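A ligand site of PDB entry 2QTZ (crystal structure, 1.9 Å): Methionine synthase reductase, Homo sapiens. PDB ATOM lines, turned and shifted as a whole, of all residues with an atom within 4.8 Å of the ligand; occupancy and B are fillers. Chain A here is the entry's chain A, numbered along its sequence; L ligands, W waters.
NE1 of Trp 538 sits close to N3 of the ligand (3.5 Å). The backbone carbonyl oxygen (O) of Val 310 is in hydrogen-bond range of a nitrogen (N2) of the ligand, at 2.8 Å. The side-chain hydroxyl of Thr 331 sits at hydrogen-bond distance from an oxygen (O14) of the ligand. OH of Tyr 294 is in hydrogen-bond range of O11 of the ligand (2.8 Å). The backbone NH of Val 329 lies within hydrogen-bond range of an oxygen (O1) of the ligand (2.9 Å). The side-chain hydroxyl (OG) of Ser 295 is in hydrogen-bond range of a nitrogen (N3) of the ligand (3.3 Å). An oxygen (O9) of the ligand is in hydrogen-bond range of the backbone carbonyl oxygen (O) of Pro 293 (2.8 Å). The backbone NH (N) of Ser 295 lies within hydrogen-bond range of an oxygen (O8) of the ligand. N of Cys 330 sits at hydrogen-bond distance from O13 of the ligand, at 2.8 Å. N of Thr 331 is in hydrogen-bond range of O14 of the ligand (2.9 Å). NE of Arg 292 is in salt-bridge range of O13 of the ligand, at 2.8 Å.
OD2 of Asp 536 sits at hydrogen-bond distance from NE1 of Trp 538, 3.3 Å away. The side-chain sulfur of Cys 330 sits close to the side-chain hydroxyl of Tyr 294 (3.5 Å). The side-chain hydroxyl (OG) of Ser 295 sits close to the indole nitrogen (NE1) of Trp 538, at 3.5 Å. The side-chain carboxylate (OD2) of Asp 536 is in hydrogen-bond range of the side-chain hydroxyl (OG) of Ser 295 (3.4 Å). The backbone NH (N) of Gly 328 is in hydrogen-bond range of the backbone carbonyl oxygen (O) of Val 314. The backbone NH (N) of Val 314 is in hydrogen-bond range of the side-chain hydroxyl (OG1) of Thr 331 (3.1 Å).
Residues that only touch the ligand: CSO 262 (3.0 Å), Phe 311 (3.2 Å), Asn 312 (3.7 Å), Val 314 (3.7 Å), Phe 316 (3.6 Å), Gly 328 (3.3 Å) and Arg 366 (3.5 Å). Hydrophobic or aromatic side chains that line the ligand: Pro 293, Tyr 294, Phe 311, Val 314, Phe 316, Val 329 and Trp 538. Of the 23 residues printed, 16 come within 4 Å of the ligand.
Water W4 lies within hydrogen-bond range of O2 of the ligand (2.6 Å) and NH2 of Arg 292 (3.4 Å). Water W11 lies within hydrogen-bond range of O7 of the ligand (2.6 Å) and O of Asn 312 (2.8 Å). Water W7 lies within hydrogen-bond range of O1 of the ligand (2.7 Å) and NH1 of Arg 218 (3.0 Å). Water W12 lies within hydrogen-bond range of O of Ser 295 (2.7 Å), O8 of the ligand (2.8 Å) and N of Val 310 (2.8 Å). Water W1 lies within hydrogen-bond range of the side-chain hydroxyl (OG1) of Thr 388 (2.6 Å), an oxygen (O7) of the ligand (2.9 Å) and the side-chain amide nitrogen (ND2) of Asn 312 (3.2 Å).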
ATOM      1  N   ALA A 153      25.502  -9.720   6.162  1.00  0.00           N
ATOM      2  CA  ALA A 153      25.134  -8.688   5.198  1.00  0.00           C
ATOM      3  C   ALA A 153      26.393  -8.117   4.551  1.00  0.00           C
ATOM      4  O   ALA A 153      27.471  -8.143   5.149  1.00  0.00           O
ATOM      5  CB  ALA A 153      24.332  -7.559   5.893  1.00  0.00           C
ATOM      6  N   ARG A 218      18.866  12.350  -4.166  1.00  0.00           N
ATOM      7  CA  ARG A 218      17.469  12.017  -3.867  1.00  0.00           C
ATOM      8  C   ARG A 218      16.964  12.520  -2.498  1.00  0.00           C
ATOM      9  O   ARG A 218      15.759  12.449  -2.221  1.00  0.00           O
ATOM     10  CB  ARG A 218      17.246  10.494  -3.931  1.00  0.00           C
ATOM     11  CG  ARG A 218      17.227   9.954  -5.379  1.00  0.00           C
ATOM     12  CD  ARG A 218      15.852  10.054  -6.007  1.00  0.00           C
ATOM     13  NE  ARG A 218      15.778   9.310  -7.265  1.00  0.00           N
ATOM     14  CZ  ARG A 218      15.458   8.024  -7.383  1.00  0.00           C
ATOM     15  NH1 ARG A 218      15.148   7.276  -6.322  1.00  0.00           N
ATOM     16  NH2 ARG A 218      15.397   7.491  -8.594  1.00  0.00           N
ATOM     17  N   CSO A 262       7.972  12.745  -1.135  1.00  0.00           N
ATOM     18  CA  CSO A 262       9.364  12.429  -1.475  1.00  0.00           C
ATOM     19  CB  CSO A 262       9.554  10.965  -1.918  1.00  0.00           C
ATOM     20  SG  CSO A 262       8.820   9.891  -0.703  1.00  0.00           S
ATOM     21  C   CSO A 262       9.984  13.371  -2.487  1.00  0.00           C
ATOM     22  O   CSO A 262      10.519  12.917  -3.498  1.00  0.00           O
ATOM     23  OD  CSO A 262      10.001   9.608   0.595  1.00  0.00           O
ATOM     24  N   ARG A 292      24.020   0.573   0.013  1.00  0.00           N
ATOM     25  CA  ARG A 292      22.837  -0.157   0.495  1.00  0.00           C
ATOM     26  C   ARG A 292      23.274  -1.565   0.884  1.00  0.00           C
ATOM     27  O   ARG A 292      23.918  -2.225   0.100  1.00  0.00           O
ATOM     28  CB  ARG A 292      21.731  -0.224  -0.590  1.00  0.00           C
ATOM     29  CG  ARG A 292      20.726   0.950  -0.616  1.00  0.00           C
ATOM     30  CD  ARG A 292      21.374   2.316  -0.928  1.00  0.00           C
ATOM     31  NE  ARG A 292      20.330   3.286  -1.342  1.00  0.00           N
ATOM     32  CZ  ARG A 292      20.501   4.604  -1.387  1.00  0.00           C
ATOM     33  NH1 ARG A 292      21.669   5.151  -1.041  1.00  0.00           N
ATOM     34  NH2 ARG A 292      19.499   5.385  -1.787  1.00  0.00           N
ATOM     35  N   PRO A 293      22.947  -2.021   2.110  1.00  0.00           N
ATOM     36  CA  PRO A 293      23.250  -3.405   2.489  1.00  0.00           C
ATOM     37  C   PRO A 293      22.263  -4.462   1.968  1.00  0.00           C
ATOM     38  O   PRO A 293      21.061  -4.172   1.816  1.00  0.00           O
ATOM     39  CB  PRO A 293      23.202  -3.347   4.028  1.00  0.00           C
ATOM     40  CG  PRO A 293      22.253  -2.280   4.317  1.00  0.00           C
ATOM     41  CD  PRO A 293      22.425  -1.243   3.239  1.00  0.00           C
ATOM     42  N   TYR A 294      22.781  -5.663   1.653  1.00  0.00           N
ATOM     43  CA  TYR A 294      21.926  -6.804   1.279  1.00  0.00           C
ATOM     44  C   TYR A 294      22.370  -8.047   2.076  1.00  0.00           C
ATOM     45  O   TYR A 294      23.541  -8.169   2.480  1.00  0.00           O
ATOM     46  CB  TYR A 294      21.939  -7.063  -0.248  1.00  0.00           C
ATOM     47  CG  TYR A 294      21.308  -5.874  -0.952  1.00  0.00           C
ATOM     48  CD1 TYR A 294      19.903  -5.801  -1.125  1.00  0.00           C
ATOM     49  CD2 TYR A 294      22.082  -4.752  -1.293  1.00  0.00           C
ATOM     50  CE1 TYR A 294      19.311  -4.643  -1.659  1.00  0.00           C
ATOM     51  CE2 TYR A 294      21.485  -3.584  -1.835  1.00  0.00           C
ATOM     52  CZ  TYR A 294      20.113  -3.551  -2.004  1.00  0.00           C
ATOM     53  OH  TYR A 294      19.509  -2.415  -2.510  1.00  0.00           O
ATOM     54  N   SER A 295      21.446  -8.989   2.251  1.00  0.00           N
ATOM     55  CA  SER A 295      21.726 -10.163   3.061  1.00  0.00           C
ATOM     56  C   SER A 295      22.250 -11.262   2.140  1.00  0.00           C
ATOM     57  O   SER A 295      21.806 -11.397   0.993  1.00  0.00           O
ATOM     58  CB  SER A 295      20.476 -10.596   3.801  1.00  0.00           C
ATOM     59  OG  SER A 295      20.000  -9.514   4.618  1.00  0.00           O
ATOM     60  N   VAL A 310      18.947 -11.301  -2.786  1.00  0.00           N
ATOM     61  CA  VAL A 310      17.563 -11.265  -3.254  1.00  0.00           C
ATOM     62  C   VAL A 310      16.997  -9.909  -2.886  1.00  0.00           C
ATOM     63  O   VAL A 310      17.142  -9.463  -1.718  1.00  0.00           O
ATOM     64  CB  VAL A 310      16.703 -12.381  -2.560  1.00  0.00           C
ATOM     65  CG1 VAL A 310      15.213 -12.264  -2.988  1.00  0.00           C
ATOM     66  CG2 VAL A 310      17.227 -13.798  -2.961  1.00  0.00           C
ATOM     67  N   PHE A 311      16.333  -9.248  -3.820  1.00  0.00           N
ATOM     68  CA  PHE A 311      15.727  -7.943  -3.487  1.00  0.00           C
ATOM     69  C   PHE A 311      14.453  -7.655  -4.315  1.00  0.00           C
ATOM     70  O   PHE A 311      14.309  -8.139  -5.424  1.00  0.00           O
ATOM     71  CB  PHE A 311      16.751  -6.780  -3.687  1.00  0.00           C
ATOM     72  CG  PHE A 311      17.286  -6.689  -5.079  1.00  0.00           C
ATOM     73  CD1 PHE A 311      16.644  -5.892  -6.045  1.00  0.00           C
ATOM     74  CD2 PHE A 311      18.401  -7.423  -5.432  1.00  0.00           C
ATOM     75  CE1 PHE A 311      17.131  -5.831  -7.352  1.00  0.00           C
ATOM     76  CE2 PHE A 311      18.891  -7.381  -6.728  1.00  0.00           C
ATOM     77  CZ  PHE A 311      18.260  -6.598  -7.693  1.00  0.00           C
ATOM     78  N   ASN A 312      13.536  -6.902  -3.714  1.00  0.00           N
ATOM     79  CA  ASN A 312      12.408  -6.308  -4.444  1.00  0.00           C
ATOM     80  C   ASN A 312      12.902  -5.020  -5.063  1.00  0.00           C
ATOM     81  O   ASN A 312      13.653  -4.227  -4.403  1.00  0.00           O
ATOM     82  CB  ASN A 312      11.252  -5.953  -3.478  1.00  0.00           C
ATOM     83  CG  ASN A 312      10.497  -7.165  -3.011  1.00  0.00           C
ATOM     84  OD1 ASN A 312      10.404  -8.172  -3.721  1.00  0.00           O
ATOM     85  ND2 ASN A 312       9.934  -7.082  -1.806  1.00  0.00           N
ATOM     86  N   VAL A 314      12.378  -1.471  -5.642  1.00  0.00           N
ATOM     87  CA  VAL A 314      11.557  -0.468  -4.918  1.00  0.00           C
ATOM     88  C   VAL A 314      10.963   0.485  -5.932  1.00  0.00           C
ATOM     89  O   VAL A 314      11.709   1.025  -6.748  1.00  0.00           O
ATOM     90  CB  VAL A 314      12.408   0.311  -3.867  1.00  0.00           C
ATOM     91  CG1 VAL A 314      11.662   1.561  -3.308  1.00  0.00           C
ATOM     92  CG2 VAL A 314      12.774  -0.614  -2.736  1.00  0.00           C
ATOM     93  N   PHE A 316       8.163   3.887  -6.039  1.00  0.00           N
ATOM     94  CA  PHE A 316       7.411   4.797  -5.187  1.00  0.00           C
ATOM     95  C   PHE A 316       6.977   6.024  -5.996  1.00  0.00           C
ATOM     96  O   PHE A 316       7.542   6.323  -7.036  1.00  0.00           O
ATOM     97  CB  PHE A 316       8.238   5.192  -3.948  1.00  0.00           C
ATOM     98  CG  PHE A 316       9.499   5.976  -4.255  1.00  0.00           C
ATOM     99  CD1 PHE A 316       9.503   7.369  -4.142  1.00  0.00           C
ATOM    100  CD2 PHE A 316      10.652   5.327  -4.741  1.00  0.00           C
ATOM    101  CE1 PHE A 316      10.653   8.128  -4.459  1.00  0.00           C
ATOM    102  CE2 PHE A 316      11.800   6.076  -5.056  1.00  0.00           C
ATOM    103  CZ  PHE A 316      11.804   7.487  -4.910  1.00  0.00           C
ATOM    104  N   GLY A 328      13.900   2.910  -6.588  1.00  0.00           N
ATOM    105  CA  GLY A 328      14.926   3.150  -5.581  1.00  0.00           C
ATOM    106  C   GLY A 328      16.271   3.290  -6.284  1.00  0.00           C
ATOM    107  O   GLY A 328      16.452   2.787  -7.408  1.00  0.00           O
ATOM    108  N   VAL A 329      17.218   3.980  -5.649  1.00  0.00           N
ATOM    109  CA  VAL A 329      18.522   4.238  -6.264  1.00  0.00           C
ATOM    110  C   VAL A 329      19.270   2.903  -6.520  1.00  0.00           C
ATOM    111  O   VAL A 329      19.688   2.609  -7.661  1.00  0.00           O
ATOM    112  CB  VAL A 329      19.362   5.167  -5.390  1.00  0.00           C
ATOM    113  CG1 VAL A 329      20.821   5.347  -5.978  1.00  0.00           C
ATOM    114  CG2 VAL A 329      18.600   6.513  -5.148  1.00  0.00           C
ATOM    115  N   CYS A 330      19.408   2.080  -5.485  1.00  0.00           N
ATOM    116  CA  CYS A 330      20.238   0.876  -5.641  1.00  0.00           C
ATOM    117  C   CYS A 330      19.469  -0.181  -6.438  1.00  0.00           C
ATOM    118  O   CYS A 330      20.000  -0.733  -7.420  1.00  0.00           O
ATOM    119  CB  CYS A 330      20.710   0.321  -4.283  1.00  0.00           C
ATOM    120  SG  CYS A 330      22.017  -0.906  -4.481  1.00  0.00           S
ATOM    121  N   THR A 331      18.222  -0.472  -6.064  1.00  0.00           N
ATOM    122  CA  THR A 331      17.491  -1.541  -6.783  1.00  0.00           C
ATOM    123  C   THR A 331      17.146  -1.164  -8.243  1.00  0.00           C
ATOM    124  O   THR A 331      17.139  -2.044  -9.122  1.00  0.00           O
ATOM    125  CB  THR A 331      16.238  -2.041  -6.013  1.00  0.00           C
ATOM    126  OG1 THR A 331      15.389  -0.925  -5.762  1.00  0.00           O
ATOM    127  CG2 THR A 331      16.654  -2.659  -4.670  1.00  0.00           C
ATOM    128  N   GLY A 332      16.919   0.124  -8.501  1.00  0.00           N
ATOM    129  CA  GLY A 332      16.690   0.606  -9.888  1.00  0.00           C
ATOM    130  C   GLY A 332      17.936   0.412 -10.747  1.00  0.00           C
ATOM    131  O   GLY A 332      17.861  -0.057 -11.890  1.00  0.00           O
ATOM    132  N   ARG A 366      30.331  -6.226   5.823  1.00  0.00           N
ATOM    133  CA  ARG A 366      30.067  -5.638   7.114  1.00  0.00           C
ATOM    134  C   ARG A 366      31.069  -6.257   8.070  1.00  0.00           C
ATOM    135  O   ARG A 366      31.466  -7.428   7.916  1.00  0.00           O
ATOM    136  CB  ARG A 366      28.620  -5.915   7.539  1.00  0.00           C
ATOM    137  CG  ARG A 366      28.149  -5.131   8.748  1.00  0.00           C
ATOM    138  CD  ARG A 366      26.636  -5.251   8.921  1.00  0.00           C
ATOM    139  NE  ARG A 366      26.229  -6.636   9.164  1.00  0.00           N
ATOM    140  CZ  ARG A 366      24.970  -7.023   9.312  1.00  0.00           C
ATOM    141  NH1 ARG A 366      23.986  -6.151   9.254  1.00  0.00           N
ATOM    142  NH2 ARG A 366      24.709  -8.305   9.528  1.00  0.00           N
ATOM    143  N   THR A 388      10.712 -11.150   0.845  1.00  0.00           N
ATOM    144  CA  THR A 388      12.163 -11.261   0.620  1.00  0.00           C
ATOM    145  C   THR A 388      12.931 -11.512   1.897  1.00  0.00           C
ATOM    146  O   THR A 388      14.118 -11.853   1.829  1.00  0.00           O
ATOM    147  CB  THR A 388      12.746 -10.035  -0.062  1.00  0.00           C
ATOM    148  OG1 THR A 388      12.309  -8.900   0.666  1.00  0.00           O
ATOM    149  CG2 THR A 388      12.222  -9.900  -1.498  1.00  0.00           C
ATOM    150  N   ALA A 391      15.247 -14.533   2.406  1.00  0.00           N
ATOM    151  CA  ALA A 391      16.591 -14.591   1.768  1.00  0.00           C
ATOM    152  C   ALA A 391      17.700 -15.272   2.592  1.00  0.00           C
ATOM    153  O   ALA A 391      18.267 -16.241   2.111  1.00  0.00           O
ATOM    154  CB  ALA A 391      17.038 -13.159   1.372  1.00  0.00           C
ATOM    155  N   ASP A 536      16.560  -9.507  11.947  1.00  0.00           N
ATOM    156  CA  ASP A 536      17.229  -8.789  10.861  1.00  0.00           C
ATOM    157  C   ASP A 536      16.165  -8.040  10.097  1.00  0.00           C
ATOM    158  O   ASP A 536      15.595  -8.553   9.135  1.00  0.00           O
ATOM    159  CB  ASP A 536      17.927  -9.768   9.929  1.00  0.00           C
ATOM    160  CG  ASP A 536      18.848  -9.084   8.898  1.00  0.00           C
ATOM    161  OD1 ASP A 536      19.271  -7.915   9.087  1.00  0.00           O
ATOM    162  OD2 ASP A 536      19.170  -9.741   7.907  1.00  0.00           O
ATOM    163  N   ILE A 537      15.906  -6.813  10.541  1.00  0.00           N
ATOM    164  CA  ILE A 537      14.802  -5.997  10.001  1.00  0.00           C
ATOM    165  C   ILE A 537      15.400  -4.884   9.137  1.00  0.00           C
ATOM    166  O   ILE A 537      16.380  -4.232   9.528  1.00  0.00           O
ATOM    167  CB  ILE A 537      13.902  -5.410  11.146  1.00  0.00           C
ATOM    168  CG1 ILE A 537      13.368  -6.540  12.056  1.00  0.00           C
ATOM    169  CG2 ILE A 537      12.739  -4.487  10.589  1.00  0.00           C
ATOM    170  CD1 ILE A 537      12.797  -7.795  11.322  1.00  0.00           C
ATOM    171  N   TRP A 538      14.801  -4.684   7.966  1.00  0.00           N
ATOM    172  CA  TRP A 538      15.481  -3.980   6.882  1.00  0.00           C
ATOM    173  C   TRP A 538      15.063  -2.537   6.738  1.00  0.00           C
ATOM    174  O   TRP A 538      15.671  -1.808   5.928  1.00  0.00           O
ATOM    175  CB  TRP A 538      15.280  -4.716   5.558  1.00  0.00           C
ATOM    176  CG  TRP A 538      15.977  -6.082   5.548  1.00  0.00           C
ATOM    177  CD1 TRP A 538      16.940  -6.506   6.393  1.00  0.00           C
ATOM    178  CD2 TRP A 538      15.780  -7.141   4.599  1.00  0.00           C
ATOM    179  NE1 TRP A 538      17.357  -7.771   6.053  1.00  0.00           N
ATOM    180  CE2 TRP A 538      16.634  -8.199   4.969  1.00  0.00           C
ATOM    181  CE3 TRP A 538      14.940  -7.306   3.502  1.00  0.00           C
ATOM    182  CZ2 TRP A 538      16.722  -9.396   4.248  1.00  0.00           C
ATOM    183  CZ3 TRP A 538      15.016  -8.496   2.795  1.00  0.00           C
ATOM    184  CH2 TRP A 538      15.891  -9.535   3.173  1.00  0.00           C
HETATM  185  P1  LIG L   1      15.990   3.943  -1.951  1.00  0.00           P
HETATM  186  O1  LIG L   1      16.258   4.918  -3.085  1.00  0.00           O
HETATM  187  O2  LIG L   1      16.914   4.055  -0.801  1.00  0.00           O
HETATM  188  O3  LIG L   1      14.495   4.165  -1.416  1.00  0.00           O
HETATM  189  C1  LIG L   1      13.440   4.909  -2.021  1.00  0.00           C
HETATM  190  C2  LIG L   1      12.828   5.545  -0.747  1.00  0.00           C
HETATM  191  O4  LIG L   1      12.208   6.829  -0.896  1.00  0.00           O
HETATM  192  C3  LIG L   1      11.858   4.653  -0.001  1.00  0.00           C
HETATM  193  O5  LIG L   1      12.504   3.700   0.809  1.00  0.00           O
HETATM  194  C4  LIG L   1      11.364   5.726   0.929  1.00  0.00           C
HETATM  195  O6  LIG L   1      12.442   6.024   1.800  1.00  0.00           O
HETATM  196  C5  LIG L   1      11.129   6.908  -0.012  1.00  0.00           C
HETATM  197  N1  LIG L   1      16.552  -5.259   1.002  1.00  0.00           N
HETATM  198  C6  LIG L   1      16.377  -6.314   0.138  1.00  0.00           C
HETATM  199  O7  LIG L   1      15.570  -6.202  -0.761  1.00  0.00           O
HETATM  200  N2  LIG L   1      17.093  -7.488   0.273  1.00  0.00           N
HETATM  201  C7  LIG L   1      18.001  -7.631   1.283  1.00  0.00           C
HETATM  202  O8  LIG L   1      18.681  -8.674   1.394  1.00  0.00           O
HETATM  203  C8  LIG L   1      18.183  -6.583   2.170  1.00  0.00           C
HETATM  204  N3  LIG L   1      19.043  -6.724   3.222  1.00  0.00           N
HETATM  205  C9  LIG L   1      19.261  -5.681   4.128  1.00  0.00           C
HETATM  206  C10 LIG L   1      20.158  -5.850   5.196  1.00  0.00           C
HETATM  207  C11 LIG L   1      20.342  -4.799   6.096  1.00  0.00           C
HETATM  208  C12 LIG L   1      21.342  -4.979   7.227  1.00  0.00           C
HETATM  209  C13 LIG L   1      19.595  -3.626   5.965  1.00  0.00           C
HETATM  210  C14 LIG L   1      19.787  -2.509   6.924  1.00  0.00           C
HETATM  211  C15 LIG L   1      18.689  -3.470   4.923  1.00  0.00           C
HETATM  212  C16 LIG L   1      18.529  -4.506   3.980  1.00  0.00           C
HETATM  213  N4  LIG L   1      17.664  -4.380   2.902  1.00  0.00           N
HETATM  214  C17 LIG L   1      17.450  -5.414   2.038  1.00  0.00           C
HETATM  215  C18 LIG L   1      17.287  -2.991   2.379  1.00  0.00           C
HETATM  216  C19 LIG L   1      18.276  -2.383   1.371  1.00  0.00           C
HETATM  217  O9  LIG L   1      19.437  -1.936   2.076  1.00  0.00           O
HETATM  218  C20 LIG L   1      17.672  -1.173   0.653  1.00  0.00           C
HETATM  219  O10 LIG L   1      17.152  -0.248   1.604  1.00  0.00           O
HETATM  220  C21 LIG L   1      16.532  -1.511  -0.318  1.00  0.00           C
HETATM  221  O11 LIG L   1      16.982  -2.337  -1.333  1.00  0.00           O
HETATM  222  C22 LIG L   1      16.029  -0.233  -1.042  1.00  0.00           C
HETATM  223  O12 LIG L   1      17.130   0.542  -1.517  1.00  0.00           O
HETATM  224  P2  LIG L   1      17.036   1.493  -2.798  1.00  0.00           P
HETATM  225  O13 LIG L   1      18.286   2.290  -2.983  1.00  0.00           O
HETATM  226  O14 LIG L   1      16.606   0.759  -4.021  1.00  0.00           O
HETATM  227  O15 LIG L   1      15.789   2.425  -2.398  1.00  0.00           O
HETATM  228  O   HOH W   1      12.771  -6.563  -0.352  1.00  0.00           O
HETATM  229  O   HOH W   2      17.634   2.429   1.320  1.00  0.00           O
HETATM  230  O   HOH W   3      14.704  -0.462   2.805  1.00  0.00           O
HETATM  231  O   HOH W   4      17.286   6.101   0.742  1.00  0.00           O
HETATM  232  O   HOH W   5      19.286  -0.055   4.136  1.00  0.00           O
HETATM  233  O   HOH W   6      13.979  -4.147   1.531  1.00  0.00           O
HETATM  234  O   HOH W   7      15.431   7.481  -3.376  1.00  0.00           O
HETATM  235  O   HOH W   8      13.689   8.860  -1.903  1.00  0.00           O
HETATM  236  O   HOH W   9      11.328   1.358   0.824  1.00  0.00           O
HETATM  237  O   HOH W  10      15.299   6.803   2.612  1.00  0.00           O
HETATM  238  O   HOH W  11      14.773  -3.927  -1.825  1.00  0.00           O
HETATM  239  O   HOH W  12      19.278 -11.079   0.025  1.00  0.00           O
